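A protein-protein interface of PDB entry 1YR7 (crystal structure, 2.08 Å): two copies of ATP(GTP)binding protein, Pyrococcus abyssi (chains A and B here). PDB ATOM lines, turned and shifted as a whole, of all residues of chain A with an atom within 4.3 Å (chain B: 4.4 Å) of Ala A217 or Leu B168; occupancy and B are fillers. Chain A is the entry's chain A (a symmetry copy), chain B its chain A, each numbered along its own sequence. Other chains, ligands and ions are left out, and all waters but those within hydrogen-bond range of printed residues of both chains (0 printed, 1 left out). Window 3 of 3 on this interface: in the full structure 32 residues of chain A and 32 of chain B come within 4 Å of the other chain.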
ATOM      1  N   ASN A 154     -13.878 -25.873 -24.637  1.00  0.00           N
ATOM      2  CA  ASN A 154     -13.384 -26.997 -23.839  1.00  0.00           C
ATOM      3  C   ASN A 154     -14.304 -28.202 -23.889  1.00  0.00           C
ATOM      4  O   ASN A 154     -13.846 -29.322 -23.697  1.00  0.00           O
ATOM      5  CB  ASN A 154     -13.046 -26.584 -22.400  1.00  0.00           C
ATOM      6  CG  ASN A 154     -14.237 -26.642 -21.469  1.00  0.00           C
ATOM      7  OD1 ASN A 154     -15.384 -26.755 -21.904  1.00  0.00           O
ATOM      8  ND2 ASN A 154     -13.968 -26.556 -20.169  1.00  0.00           N
ATOM      9  N   CYS A 157     -12.700 -30.367 -26.229  1.00  0.00           N
ATOM     10  CA  CYS A 157     -11.592 -31.062 -25.571  1.00  0.00           C
ATOM     11  C   CYS A 157     -12.104 -32.163 -24.623  1.00  0.00           C
ATOM     12  O   CYS A 157     -11.488 -33.225 -24.456  1.00  0.00           O
ATOM     13  CB  CYS A 157     -10.754 -30.044 -24.788  1.00  0.00           C
ATOM     14  SG  CYS A 157      -9.336 -30.768 -23.931  1.00  0.00           S
ATOM     15  N   LEU A 206      -8.567 -21.601 -27.182  1.00  0.00           N
ATOM     16  CA  LEU A 206      -8.259 -21.956 -25.801  1.00  0.00           C
ATOM     17  C   LEU A 206      -7.199 -21.017 -25.242  1.00  0.00           C
ATOM     18  O   LEU A 206      -7.057 -20.877 -24.027  1.00  0.00           O
ATOM     19  CB  LEU A 206      -7.770 -23.406 -25.708  1.00  0.00           C
ATOM     20  CG  LEU A 206      -8.785 -24.526 -25.964  1.00  0.00           C
ATOM     21  CD1 LEU A 206      -8.138 -25.892 -25.789  1.00  0.00           C
ATOM     22  CD2 LEU A 206     -10.005 -24.383 -25.061  1.00  0.00           C
ATOM     23  N   GLY A 214      -9.713 -23.432 -19.147  1.00  0.00           N
ATOM     24  CA  GLY A 214      -9.525 -22.897 -20.493  1.00  0.00           C
ATOM     25  C   GLY A 214      -8.037 -22.857 -20.770  1.00  0.00           C
ATOM     26  O   GLY A 214      -7.563 -23.403 -21.769  1.00  0.00           O
ATOM     27  N   LEU A 215      -7.303 -22.199 -19.878  1.00  0.00           N
ATOM     28  CA  LEU A 215      -5.868 -22.389 -19.800  1.00  0.00           C
ATOM     29  C   LEU A 215      -5.703 -23.860 -19.466  1.00  0.00           C
ATOM     30  O   LEU A 215      -4.968 -24.589 -20.135  1.00  0.00           O
ATOM     31  CB  LEU A 215      -5.261 -21.510 -18.704  1.00  0.00           C
ATOM     32  CG  LEU A 215      -3.802 -21.748 -18.303  1.00  0.00           C
ATOM     33  CD1 LEU A 215      -3.091 -20.431 -18.030  1.00  0.00           C
ATOM     34  CD2 LEU A 215      -3.706 -22.678 -17.099  1.00  0.00           C
ATOM     35  N   MET A 216      -6.413 -24.284 -18.425  1.00  0.00           N
ATOM     36  CA  MET A 216      -6.560 -25.695 -18.113  1.00  0.00           C
ATOM     37  C   MET A 216      -7.448 -26.324 -19.175  1.00  0.00           C
ATOM     38  O   MET A 216      -8.673 -26.263 -19.089  1.00  0.00           O
ATOM     39  CB  MET A 216      -7.183 -25.876 -16.735  1.00  0.00           C
ATOM     40  CG  MET A 216      -6.414 -25.209 -15.619  1.00  0.00           C
ATOM     41  SD  MET A 216      -6.937 -25.826 -14.016  1.00  0.00           S
ATOM     42  CE  MET A 216      -6.088 -27.403 -13.964  1.00  0.00           C
ATOM     43  N   ALA A 217      -6.802 -26.923 -20.173  1.00  0.00           N
ATOM     44  CA  ALA A 217      -7.452 -27.408 -21.385  1.00  0.00           C
ATOM     45  C   ALA A 217      -6.554 -27.058 -22.563  1.00  0.00           C
ATOM     46  O   ALA A 217      -6.338 -27.872 -23.462  1.00  0.00           O
ATOM     47  CB  ALA A 217      -8.797 -26.777 -21.556  1.00  0.00           C
ATOM     48  N   TYR A 218      -6.040 -25.829 -22.548  1.00  0.00           N
ATOM     49  CA  TYR A 218      -5.010 -25.397 -23.485  1.00  0.00           C
ATOM     50  C   TYR A 218      -3.764 -26.202 -23.177  1.00  0.00           C
ATOM     51  O   TYR A 218      -3.282 -26.962 -24.020  1.00  0.00           O
ATOM     52  CB  TYR A 218      -4.735 -23.897 -23.320  1.00  0.00           C
ATOM     53  CG  TYR A 218      -3.658 -23.334 -24.227  1.00  0.00           C
ATOM     54  CD1 TYR A 218      -2.322 -23.332 -23.837  1.00  0.00           C
ATOM     55  CD2 TYR A 218      -3.979 -22.782 -25.460  1.00  0.00           C
ATOM     56  CE1 TYR A 218      -1.336 -22.812 -24.657  1.00  0.00           C
ATOM     57  CE2 TYR A 218      -2.999 -22.257 -26.289  1.00  0.00           C
ATOM     58  CZ  TYR A 218      -1.680 -22.276 -25.881  1.00  0.00           C
ATOM     59  OH  TYR A 218      -0.703 -21.756 -26.700  1.00  0.00           O
ATOM     60  N   LYS A 219      -3.265 -26.059 -21.950  1.00  0.00           N
ATOM     61  CA  LYS A 219      -2.103 -26.823 -21.505  1.00  0.00           C
ATOM     62  C   LYS A 219      -2.334 -28.326 -21.589  1.00  0.00           C
ATOM     63  O   LYS A 219      -1.380 -29.104 -21.680  1.00  0.00           O
ATOM     64  CB  LYS A 219      -1.675 -26.426 -20.088  1.00  0.00           C
ATOM     65  CG  LYS A 219      -0.500 -25.457 -20.054  1.00  0.00           C
ATOM     66  CD  LYS A 219       0.497 -25.837 -18.963  1.00  0.00           C
ATOM     67  CE  LYS A 219       1.901 -25.351 -19.309  1.00  0.00           C
ATOM     68  NZ  LYS A 219       2.923 -25.809 -18.325  1.00  0.00           N
ATOM     69  N   MET A 220      -3.601 -28.731 -21.561  1.00  0.00           N
ATOM     70  CA  MET A 220      -3.956 -30.138 -21.703  1.00  0.00           C
ATOM     71  C   MET A 220      -3.741 -30.605 -23.136  1.00  0.00           C
ATOM     72  O   MET A 220      -2.682 -31.134 -23.480  1.00  0.00           O
ATOM     73  CB  MET A 220      -5.417 -30.362 -21.322  1.00  0.00           C
ATOM     74  CG  MET A 220      -5.687 -30.411 -19.834  1.00  0.00           C
ATOM     75  SD  MET A 220      -7.209 -31.315 -19.515  1.00  0.00           S
ATOM     76  CE  MET A 220      -6.808 -32.878 -20.298  1.00  0.00           C
ATOM     77  N   CYS A 221      -4.764 -30.378 -23.957  1.00  0.00           N
ATOM     78  CA  CYS A 221      -4.809 -30.782 -25.362  1.00  0.00           C
ATOM     79  C   CYS A 221      -3.590 -30.325 -26.156  1.00  0.00           C
ATOM     80  O   CYS A 221      -3.316 -30.851 -27.240  1.00  0.00           O
ATOM     81  CB  CYS A 221      -6.081 -30.216 -26.004  1.00  0.00           C
ATOM     82  SG  CYS A 221      -6.588 -30.997 -27.544  1.00  0.00           S
ATOM     83  N   LEU B 164      -9.822 -34.676 -13.506  1.00  0.00           N
ATOM     84  CA  LEU B 164      -9.364 -33.632 -14.411  1.00  0.00           C
ATOM     85  C   LEU B 164     -10.482 -33.268 -15.390  1.00  0.00           C
ATOM     86  O   LEU B 164     -10.756 -32.086 -15.663  1.00  0.00           O
ATOM     87  CB  LEU B 164      -8.142 -34.146 -15.169  1.00  0.00           C
ATOM     88  CG  LEU B 164      -7.077 -33.098 -15.441  1.00  0.00           C
ATOM     89  CD1 LEU B 164      -5.680 -33.612 -15.055  1.00  0.00           C
ATOM     90  CD2 LEU B 164      -7.131 -32.635 -16.893  1.00  0.00           C
ATOM     91  N   LEU B 165     -11.134 -34.305 -15.896  1.00  0.00           N
ATOM     92  CA  LEU B 165     -12.246 -34.173 -16.834  1.00  0.00           C
ATOM     93  C   LEU B 165     -13.473 -33.498 -16.225  1.00  0.00           C
ATOM     94  O   LEU B 165     -14.077 -32.612 -16.842  1.00  0.00           O
ATOM     95  CB  LEU B 165     -12.631 -35.568 -17.349  1.00  0.00           C
ATOM     96  CG  LEU B 165     -14.042 -35.801 -17.897  1.00  0.00           C
ATOM     97  CD1 LEU B 165     -14.335 -34.922 -19.091  1.00  0.00           C
ATOM     98  CD2 LEU B 165     -14.215 -37.257 -18.266  1.00  0.00           C
ATOM     99  N   ILE B 166     -13.843 -33.918 -15.017  1.00  0.00           N
ATOM    100  CA  ILE B 166     -14.918 -33.265 -14.291  1.00  0.00           C
ATOM    101  C   ILE B 166     -14.542 -31.805 -14.160  1.00  0.00           C
ATOM    102  O   ILE B 166     -15.354 -30.895 -14.376  1.00  0.00           O
ATOM    103  CB  ILE B 166     -15.103 -33.919 -12.891  1.00  0.00           C
ATOM    104  CG1 ILE B 166     -15.725 -35.320 -13.028  1.00  0.00           C
ATOM    105  CG2 ILE B 166     -15.946 -33.050 -11.996  1.00  0.00           C
ATOM    106  CD1 ILE B 166     -15.514 -36.210 -11.811  1.00  0.00           C
ATOM    107  N   ASP B 167     -13.286 -31.588 -13.794  1.00  0.00           N
ATOM    108  CA  ASP B 167     -12.727 -30.253 -13.647  1.00  0.00           C
ATOM    109  C   ASP B 167     -12.884 -29.480 -14.975  1.00  0.00           C
ATOM    110  O   ASP B 167     -13.352 -28.335 -15.015  1.00  0.00           O
ATOM    111  CB  ASP B 167     -11.250 -30.419 -13.268  1.00  0.00           C
ATOM    112  CG  ASP B 167     -10.610 -29.157 -12.756  1.00  0.00           C
ATOM    113  OD1 ASP B 167     -10.773 -28.080 -13.383  1.00  0.00           O
ATOM    114  OD2 ASP B 167      -9.900 -29.255 -11.733  1.00  0.00           O
ATOM    115  N   LEU B 168     -12.483 -30.107 -16.069  1.00  0.00           N
ATOM    116  CA  LEU B 168     -12.636 -29.475 -17.373  1.00  0.00           C
ATOM    117  C   LEU B 168     -14.113 -29.132 -17.591  1.00  0.00           C
ATOM    118  O   LEU B 168     -14.487 -27.972 -17.777  1.00  0.00           O
ATOM    119  CB  LEU B 168     -12.155 -30.433 -18.466  1.00  0.00           C
ATOM    120  CG  LEU B 168     -11.780 -29.853 -19.823  1.00  0.00           C
ATOM    121  CD1 LEU B 168     -11.196 -28.460 -19.672  1.00  0.00           C
ATOM    122  CD2 LEU B 168     -10.796 -30.783 -20.485  1.00  0.00           C
ATOM    123  N   ARG B 169     -14.945 -30.162 -17.521  1.00  0.00           N
ATOM    124  CA  ARG B 169     -16.370 -30.071 -17.819  1.00  0.00           C
ATOM    125  C   ARG B 169     -17.199 -29.095 -16.950  1.00  0.00           C
ATOM    126  O   ARG B 169     -18.116 -28.435 -17.462  1.00  0.00           O
ATOM    127  CB  ARG B 169     -16.955 -31.486 -17.760  1.00  0.00           C
ATOM    128  CG  ARG B 169     -18.435 -31.591 -18.084  1.00  0.00           C
ATOM    129  CD  ARG B 169     -18.741 -31.137 -19.510  1.00  0.00           C
ATOM    130  NE  ARG B 169     -20.174 -31.186 -19.722  1.00  0.00           N
ATOM    131  CZ  ARG B 169     -20.805 -30.636 -20.751  1.00  0.00           C
ATOM    132  NH1 ARG B 169     -20.128 -29.975 -21.678  1.00  0.00           N
ATOM    133  NH2 ARG B 169     -22.127 -30.747 -20.843  1.00  0.00           N
ATOM    134  N   LEU B 170     -16.912 -29.013 -15.648  1.00  0.00           N
ATOM    135  CA  LEU B 170     -17.693 -28.157 -14.750  1.00  0.00           C
ATOM    136  C   LEU B 170     -17.002 -26.832 -14.480  1.00  0.00           C
ATOM    137  O   LEU B 170     -17.609 -25.909 -13.939  1.00  0.00           O
ATOM    138  CB  LEU B 170     -18.009 -28.864 -13.413  1.00  0.00           C
ATOM    139  CG  LEU B 170     -18.754 -30.207 -13.453  1.00  0.00           C
ATOM    140  CD1 LEU B 170     -18.695 -30.915 -12.104  1.00  0.00           C
ATOM    141  CD2 LEU B 170     -20.210 -30.015 -13.930  1.00  0.00           C
ATOM    142  N   GLY B 171     -15.729 -26.730 -14.839  1.00  0.00           N
ATOM    143  CA  GLY B 171     -14.973 -25.491 -14.578  1.00  0.00           C
ATOM    144  C   GLY B 171     -14.896 -25.183 -13.087  1.00  0.00           C
ATOM    145  O   GLY B 171     -15.155 -24.061 -12.641  1.00  0.00           O
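The side-chain amide nitrogen of Asn A154 sits at hydrogen-bond distance from the backbone carbonyl oxygen of Leu B168, at 2.8 Å.
SG of Cys A157 touches CD2 of Leu B168, 3.7 Å away. Leu B168 touches Met A216. Leu B168 touches Ala A217 (CD1 to CB, 3.5 Å). Met A220 touches Leu B164. Leu B168 touches Met A220.
Printed residues of chain B within 4 Å of Asn A154: Leu B168 (2.8 Å). Printed residues of chain B within 4 Å of Cys A157: Leu B168. Printed residues of chain B within 4 Å of Met A216: Leu B168 (3.4 Å). Ala A217 touches one residue of chain B. Of the printed residues of chain B, Met A220 touches Leu B164 (2.9 Å) and Leu B168 (3.8 Å). Cys A221 touches none of the printed residues of chain B. Printed residues of chain A within 4 Å of Leu B164: Met A220. Ile B166 touches none of the printed residues of chain A. Printed residues of chain A within 4 Å of Leu B168: Asn A154 (2.8 Å), Cys A157 (3.7 Å), Met A216 (3.4 Å), Ala A217 (3.5 Å) and Met A220 (3.8 Å). The nearest printed residue of chain B that does not touch Ala A217 is Leu B164 (6.6 Å). The nearest printed residue of chain A that does not touch Leu B168 is Gly A214 (5.3 Å). The nearest printed residue of chain A that does not touch Leu B164 is Met A216 (6.0 Å).
Of the 8 printed residues of chain B, 2 touch a printed residue of chain A. Hydrophobic or aromatic side chains of chain B that line the printed part of chain A: Leu B164 and Leu B168. Along chain B the printed residues that touch a printed residue of chain A span positions 164 to 168. Of the 11 printed residues of chain A, 5 touch a printed residue of chain B. Hydrophobic or aromatic side chains of chain A within 4 Å of the printed part of chain B: Ala A217 and Met A220. Among the printed residues, 6 pairs touch across the chains. Among the printed residues, no Asp or Glu carboxylate lies within 4 Å of a Lys or Arg side-chain nitrogen of the other chain.
No position is printed for both chains. Of the 6 pairs that touch across the chains among the printed residues, none has its exchanged pair printed and touching as well.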
